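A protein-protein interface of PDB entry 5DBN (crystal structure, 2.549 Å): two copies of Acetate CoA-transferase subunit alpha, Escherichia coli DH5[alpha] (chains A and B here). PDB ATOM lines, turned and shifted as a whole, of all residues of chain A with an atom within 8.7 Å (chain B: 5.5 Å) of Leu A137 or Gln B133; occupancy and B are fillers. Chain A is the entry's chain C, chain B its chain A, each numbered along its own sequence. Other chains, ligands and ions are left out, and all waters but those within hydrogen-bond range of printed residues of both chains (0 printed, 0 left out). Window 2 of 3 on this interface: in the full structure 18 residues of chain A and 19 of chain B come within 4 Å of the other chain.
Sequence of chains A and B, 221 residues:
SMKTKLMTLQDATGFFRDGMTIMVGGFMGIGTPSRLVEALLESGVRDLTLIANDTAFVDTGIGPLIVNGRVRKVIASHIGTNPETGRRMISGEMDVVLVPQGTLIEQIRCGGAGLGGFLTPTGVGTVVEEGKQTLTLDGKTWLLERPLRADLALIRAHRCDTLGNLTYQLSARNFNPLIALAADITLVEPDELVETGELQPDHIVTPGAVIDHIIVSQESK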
ATOM      1  N   LEU A 119     -12.767 -11.285  21.177  1.00  0.00           N
ATOM      2  CA  LEU A 119     -13.542 -12.491  21.453  1.00  0.00           C
ATOM      3  C   LEU A 119     -12.841 -13.708  20.856  1.00  0.00           C
ATOM      4  O   LEU A 119     -12.516 -13.724  19.668  1.00  0.00           O
ATOM      5  CB  LEU A 119     -14.959 -12.361  20.888  1.00  0.00           C
ATOM      6  CG  LEU A 119     -15.766 -11.153  21.376  1.00  0.00           C
ATOM      7  CD1 LEU A 119     -17.136 -11.119  20.715  1.00  0.00           C
ATOM      8  CD2 LEU A 119     -15.913 -11.173  22.892  1.00  0.00           C
ATOM      9  N   THR A 134     -18.092 -14.012  29.277  1.00  0.00           N
ATOM     10  CA  THR A 134     -18.428 -14.795  28.098  1.00  0.00           C
ATOM     11  C   THR A 134     -19.573 -14.126  27.347  1.00  0.00           C
ATOM     12  O   THR A 134     -20.540 -13.666  27.953  1.00  0.00           O
ATOM     13  CB  THR A 134     -18.832 -16.229  28.467  1.00  0.00           C
ATOM     14  OG1 THR A 134     -20.080 -16.211  29.169  1.00  0.00           O
ATOM     15  CG2 THR A 134     -17.770 -16.873  29.338  1.00  0.00           C
ATOM     16  N   LEU A 135     -19.448 -14.069  26.025  1.00  0.00           N
ATOM     17  CA  LEU A 135     -20.464 -13.473  25.163  1.00  0.00           C
ATOM     18  C   LEU A 135     -20.995 -14.481  24.151  1.00  0.00           C
ATOM     19  O   LEU A 135     -20.242 -15.301  23.624  1.00  0.00           O
ATOM     20  CB  LEU A 135     -19.891 -12.255  24.433  1.00  0.00           C
ATOM     21  CG  LEU A 135     -19.857 -10.936  25.208  1.00  0.00           C
ATOM     22  CD1 LEU A 135     -18.824 -10.948  26.321  1.00  0.00           C
ATOM     23  CD2 LEU A 135     -19.572  -9.790  24.252  1.00  0.00           C
ATOM     24  N   THR A 136     -22.296 -14.413  23.883  1.00  0.00           N
ATOM     25  CA  THR A 136     -22.922 -15.271  22.885  1.00  0.00           C
ATOM     26  C   THR A 136     -23.165 -14.477  21.601  1.00  0.00           C
ATOM     27  O   THR A 136     -23.849 -13.454  21.610  1.00  0.00           O
ATOM     28  CB  THR A 136     -24.254 -15.858  23.398  1.00  0.00           C
ATOM     29  OG1 THR A 136     -24.032 -16.560  24.628  1.00  0.00           O
ATOM     30  CG2 THR A 136     -24.858 -16.811  22.375  1.00  0.00           C
ATOM     31  N   LEU A 137     -22.592 -14.965  20.506  1.00  0.00           N
ATOM     32  CA  LEU A 137     -22.692 -14.321  19.199  1.00  0.00           C
ATOM     33  C   LEU A 137     -22.736 -15.381  18.104  1.00  0.00           C
ATOM     34  O   LEU A 137     -21.876 -16.260  18.063  1.00  0.00           O
ATOM     35  CB  LEU A 137     -21.524 -13.366  18.963  1.00  0.00           C
ATOM     36  CG  LEU A 137     -21.585 -11.992  19.638  1.00  0.00           C
ATOM     37  CD1 LEU A 137     -20.385 -11.161  19.230  1.00  0.00           C
ATOM     38  CD2 LEU A 137     -22.874 -11.249  19.314  1.00  0.00           C
ATOM     39  N   ASP A 138     -23.746 -15.304  17.237  1.00  0.00           N
ATOM     40  CA  ASP A 138     -23.928 -16.264  16.147  1.00  0.00           C
ATOM     41  C   ASP A 138     -24.263 -17.646  16.695  1.00  0.00           C
ATOM     42  O   ASP A 138     -24.115 -18.652  16.002  1.00  0.00           O
ATOM     43  CB  ASP A 138     -22.678 -16.342  15.262  1.00  0.00           C
ATOM     44  CG  ASP A 138     -22.322 -15.010  14.646  1.00  0.00           C
ATOM     45  OD1 ASP A 138     -23.190 -14.109  14.642  1.00  0.00           O
ATOM     46  OD2 ASP A 138     -21.174 -14.850  14.178  1.00  0.00           O
ATOM     47  N   GLY A 139     -24.712 -17.684  17.946  1.00  0.00           N
ATOM     48  CA  GLY A 139     -25.079 -18.926  18.598  1.00  0.00           C
ATOM     49  C   GLY A 139     -23.858 -19.573  19.225  1.00  0.00           C
ATOM     50  O   GLY A 139     -23.949 -20.644  19.827  1.00  0.00           O
ATOM     51  N   LYS A 140     -22.713 -18.911  19.072  1.00  0.00           N
ATOM     52  CA  LYS A 140     -21.444 -19.405  19.585  1.00  0.00           C
ATOM     53  C   LYS A 140     -20.991 -18.607  20.805  1.00  0.00           C
ATOM     54  O   LYS A 140     -21.138 -17.384  20.844  1.00  0.00           O
ATOM     55  CB  LYS A 140     -20.381 -19.347  18.495  1.00  0.00           C
ATOM     56  CG  LYS A 140     -19.060 -19.922  18.925  1.00  0.00           C
ATOM     57  CD  LYS A 140     -18.059 -19.909  17.800  1.00  0.00           C
ATOM     58  CE  LYS A 140     -16.745 -20.430  18.308  1.00  0.00           C
ATOM     59  NZ  LYS A 140     -15.665 -20.442  17.284  1.00  0.00           N
ATOM     60  N   THR A 141     -20.439 -19.305  21.794  1.00  0.00           N
ATOM     61  CA  THR A 141     -19.935 -18.666  23.005  1.00  0.00           C
ATOM     62  C   THR A 141     -18.470 -18.276  22.832  1.00  0.00           C
ATOM     63  O   THR A 141     -17.662 -19.070  22.349  1.00  0.00           O
ATOM     64  CB  THR A 141     -20.076 -19.594  24.232  1.00  0.00           C
ATOM     65  OG1 THR A 141     -21.455 -19.935  24.419  1.00  0.00           O
ATOM     66  CG2 THR A 141     -19.547 -18.917  25.495  1.00  0.00           C
ATOM     67  N   TRP A 142     -18.139 -17.055  23.242  1.00  0.00           N
ATOM     68  CA  TRP A 142     -16.778 -16.533  23.138  1.00  0.00           C
ATOM     69  C   TRP A 142     -16.275 -16.045  24.491  1.00  0.00           C
ATOM     70  O   TRP A 142     -17.033 -15.471  25.267  1.00  0.00           O
ATOM     71  CB  TRP A 142     -16.709 -15.371  22.145  1.00  0.00           C
ATOM     72  CG  TRP A 142     -17.373 -15.606  20.823  1.00  0.00           C
ATOM     73  CD1 TRP A 142     -18.704 -15.503  20.542  1.00  0.00           C
ATOM     74  CD2 TRP A 142     -16.728 -15.950  19.591  1.00  0.00           C
ATOM     75  NE1 TRP A 142     -18.929 -15.774  19.214  1.00  0.00           N
ATOM     76  CE2 TRP A 142     -17.732 -16.050  18.608  1.00  0.00           C
ATOM     77  CE3 TRP A 142     -15.400 -16.189  19.224  1.00  0.00           C
ATOM     78  CZ2 TRP A 142     -17.451 -16.381  17.284  1.00  0.00           C
ATOM     79  CZ3 TRP A 142     -15.123 -16.518  17.910  1.00  0.00           C
ATOM     80  CH2 TRP A 142     -16.145 -16.610  16.956  1.00  0.00           C
ATOM     81  N   GLY B 116     -14.107 -13.671  17.125  1.00  0.00           N
ATOM     82  CA  GLY B 116     -15.531 -13.381  17.095  1.00  0.00           C
ATOM     83  C   GLY B 116     -15.865 -11.901  17.082  1.00  0.00           C
ATOM     84  O   GLY B 116     -17.032 -11.528  16.962  1.00  0.00           O
ATOM     85  N   GLU B 129     -21.411   4.393  15.558  1.00  0.00           N
ATOM     86  CA  GLU B 129     -21.905   3.674  16.732  1.00  0.00           C
ATOM     87  C   GLU B 129     -23.285   3.052  16.522  1.00  0.00           C
ATOM     88  O   GLU B 129     -23.651   2.092  17.203  1.00  0.00           O
ATOM     89  CB  GLU B 129     -21.961   4.625  17.932  1.00  0.00           C
ATOM     90  CG  GLU B 129     -22.474   3.987  19.213  1.00  0.00           C
ATOM     91  CD  GLU B 129     -22.395   4.919  20.406  1.00  0.00           C
ATOM     92  OE1 GLU B 129     -23.279   4.828  21.284  1.00  0.00           O
ATOM     93  OE2 GLU B 129     -21.454   5.737  20.470  1.00  0.00           O
ATOM     94  N   GLY B 131     -26.358   0.955  15.666  1.00  0.00           N
ATOM     95  CA  GLY B 131     -26.608  -0.441  15.357  1.00  0.00           C
ATOM     96  C   GLY B 131     -25.535  -1.380  15.879  1.00  0.00           C
ATOM     97  O   GLY B 131     -25.551  -2.574  15.570  1.00  0.00           O
ATOM     98  N   LYS B 132     -24.599  -0.846  16.661  1.00  0.00           N
ATOM     99  CA  LYS B 132     -23.492  -1.634  17.198  1.00  0.00           C
ATOM    100  C   LYS B 132     -23.532  -1.701  18.718  1.00  0.00           C
ATOM    101  O   LYS B 132     -24.089  -0.824  19.377  1.00  0.00           O
ATOM    102  CB  LYS B 132     -22.157  -1.053  16.732  1.00  0.00           C
ATOM    103  CG  LYS B 132     -21.959  -1.159  15.233  1.00  0.00           C
ATOM    104  CD  LYS B 132     -20.641  -0.585  14.798  1.00  0.00           C
ATOM    105  CE  LYS B 132     -20.498  -0.651  13.292  1.00  0.00           C
ATOM    106  NZ  LYS B 132     -19.340   0.144  12.809  1.00  0.00           N
ATOM    107  N   GLN B 133     -22.935  -2.755  19.266  1.00  0.00           N
ATOM    108  CA  GLN B 133     -22.842  -2.927  20.708  1.00  0.00           C
ATOM    109  C   GLN B 133     -21.713  -2.079  21.263  1.00  0.00           C
ATOM    110  O   GLN B 133     -20.636  -2.015  20.671  1.00  0.00           O
ATOM    111  CB  GLN B 133     -22.592  -4.392  21.070  1.00  0.00           C
ATOM    112  CG  GLN B 133     -23.806  -5.292  20.991  1.00  0.00           C
ATOM    113  CD  GLN B 133     -23.502  -6.706  21.456  1.00  0.00           C
ATOM    114  OE1 GLN B 133     -23.800  -7.679  20.760  1.00  0.00           O
ATOM    115  NE2 GLN B 133     -22.904  -6.827  22.638  1.00  0.00           N
ATOM    116  N   THR B 134     -21.962  -1.432  22.397  1.00  0.00           N
ATOM    117  CA  THR B 134     -20.935  -0.644  23.062  1.00  0.00           C
ATOM    118  C   THR B 134     -20.653  -1.266  24.422  1.00  0.00           C
ATOM    119  O   THR B 134     -21.577  -1.566  25.172  1.00  0.00           O
ATOM    120  CB  THR B 134     -21.366   0.823  23.241  1.00  0.00           C
ATOM    121  OG1 THR B 134     -22.455   0.895  24.170  1.00  0.00           O
ATOM    122  CG2 THR B 134     -21.801   1.421  21.914  1.00  0.00           C
ATOM    123  N   LEU B 135     -19.374  -1.432  24.739  1.00  0.00           N
ATOM    124  CA  LEU B 135     -18.946  -2.016  26.008  1.00  0.00           C
ATOM    125  C   LEU B 135     -18.057  -1.061  26.778  1.00  0.00           C
ATOM    126  O   LEU B 135     -17.254  -0.343  26.185  1.00  0.00           O
ATOM    127  CB  LEU B 135     -18.197  -3.329  25.773  1.00  0.00           C
ATOM    128  CG  LEU B 135     -19.012  -4.603  25.543  1.00  0.00           C
ATOM    129  CD1 LEU B 135     -19.708  -4.594  24.191  1.00  0.00           C
ATOM    130  CD2 LEU B 135     -18.103  -5.818  25.659  1.00  0.00           C
ATOM    131  N   TRP B 142     -16.091   1.293  24.335  1.00  0.00           N
ATOM    132  CA  TRP B 142     -15.586   0.690  23.103  1.00  0.00           C
ATOM    133  C   TRP B 142     -16.739   0.248  22.217  1.00  0.00           C
ATOM    134  O   TRP B 142     -17.759  -0.224  22.715  1.00  0.00           O
ATOM    135  CB  TRP B 142     -14.708  -0.528  23.403  1.00  0.00           C
ATOM    136  CG  TRP B 142     -13.686  -0.328  24.474  1.00  0.00           C
ATOM    137  CD1 TRP B 142     -13.893  -0.384  25.819  1.00  0.00           C
ATOM    138  CD2 TRP B 142     -12.291  -0.066  24.291  1.00  0.00           C
ATOM    139  NE1 TRP B 142     -12.715  -0.162  26.488  1.00  0.00           N
ATOM    140  CE2 TRP B 142     -11.715   0.034  25.572  1.00  0.00           C
ATOM    141  CE3 TRP B 142     -11.473   0.099  23.170  1.00  0.00           C
ATOM    142  CZ2 TRP B 142     -10.360   0.293  25.764  1.00  0.00           C
ATOM    143  CZ3 TRP B 142     -10.127   0.356  23.363  1.00  0.00           C
ATOM    144  CH2 TRP B 142      -9.585   0.451  24.649  1.00  0.00           C
ATOM    145  N   LEU B 143     -16.583   0.404  20.906  1.00  0.00           N
ATOM    146  CA  LEU B 143     -17.503  -0.220  19.965  1.00  0.00           C
ATOM    147  C   LEU B 143     -17.075  -1.656  19.735  1.00  0.00           C
ATOM    148  O   LEU B 143     -15.906  -1.922  19.455  1.00  0.00           O
ATOM    149  CB  LEU B 143     -17.547   0.532  18.633  1.00  0.00           C
ATOM    150  CG  LEU B 143     -17.963   2.005  18.649  1.00  0.00           C
ATOM    151  CD1 LEU B 143     -18.221   2.473  17.226  1.00  0.00           C
ATOM    152  CD2 LEU B 143     -19.195   2.234  19.517  1.00  0.00           C
ATOM    153  N   LEU B 144     -18.021  -2.578  19.851  1.00  0.00           N
ATOM    154  CA  LEU B 144     -17.760  -3.975  19.537  1.00  0.00           C
ATOM    155  C   LEU B 144     -17.968  -4.205  18.046  1.00  0.00           C
ATOM    156  O   LEU B 144     -19.094  -4.158  17.553  1.00  0.00           O
ATOM    157  CB  LEU B 144     -18.667  -4.898  20.353  1.00  0.00           C
ATOM    158  CG  LEU B 144     -18.532  -6.397  20.065  1.00  0.00           C
ATOM    159  CD1 LEU B 144     -17.111  -6.885  20.289  1.00  0.00           C
ATOM    160  CD2 LEU B 144     -19.505  -7.183  20.924  1.00  0.00           C
ATOM    161  N   ARG B 146     -17.536  -6.560  14.538  1.00  0.00           N
ATOM    162  CA  ARG B 146     -17.715  -7.968  14.214  1.00  0.00           C
ATOM    163  C   ARG B 146     -16.884  -8.358  12.992  1.00  0.00           C
ATOM    164  O   ARG B 146     -16.564  -7.506  12.163  1.00  0.00           O
ATOM    165  CB  ARG B 146     -19.202  -8.232  13.962  1.00  0.00           C
ATOM    166  CG  ARG B 146     -20.086  -7.858  15.147  1.00  0.00           C
ATOM    167  CD  ARG B 146     -20.180  -8.959  16.182  1.00  0.00           C
ATOM    168  NE  ARG B 146     -21.267  -9.877  15.845  1.00  0.00           N
ATOM    169  CZ  ARG B 146     -21.138 -11.180  15.606  1.00  0.00           C
ATOM    170  NH1 ARG B 146     -19.956 -11.784  15.659  1.00  0.00           N
ATOM    171  NH2 ARG B 146     -22.218 -11.886  15.308  1.00  0.00           N
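3 positions are printed for both chains. Of the 5 pairs that touch across the chains among the printed residues, none has its exchanged pair printed and touching as well.
The backbone carbonyl oxygen of Gly B116 lies within hydrogen-bond range of the guanidinium group of Arg B146. O of Gln B133 sits at hydrogen-bond distance from N of Leu B144 (2.8 Å). O of Leu A135 is in hydrogen-bond range of N of Trp A142 (2.8 Å). NE1 of Trp A142 is in hydrogen-bond range of O of Leu A137, at 3.2 Å. The backbone carbonyl oxygen (O) of Lys A140 sits close to the indole nitrogen (NE1) of Trp A142 (3.2 Å).
Printed residues of chain B within 4 Å of Leu A119: Gly B116 (3.0 Å). Thr A136 touches none of the printed residues of chain B. Of chain B, only Gln B133 (3.96 Å) and Arg B146 (3.7 Å) come within 4 Å of Leu A137. Printed residues of chain B within 4 Å of Asp A138: Arg B146 (2.5 Å). No residue of chain A comes within 4 Å of Thr B134. The nearest residue of chain B that does not touch Leu A137 is Gly B116 (4.1 Å).
Printed residues of chain B that touch a printed residue of chain A: Gly B116, Gln B133 and Arg B146. Hydrophobic or aromatic side chains of chain A that line the printed part of chain B: Leu A119, Leu A137 and Trp A142. Among the printed residues, Asp or Glu carboxylates within 4 Å of a Lys or Arg side-chain nitrogen of the other chain: Asp A138 with Arg B146 (2.5 Å).
The backbone NH (N) of Gly B116 lies within hydrogen-bond range of the backbone carbonyl oxygen (O) of Leu A119. The guanidinium group (NH2) of Arg B146 lies within salt-bridge range of the side-chain carboxylate (OD1) of Asp A138 (2.5 Å).
Among the printed residues, pairs that only touch across the chains: Leu A137 with Gln B133 (3.96 Å), Leu A137 with Arg B146 (3.7 Å) and Trp A142 with Gly B116 (3.1 Å).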
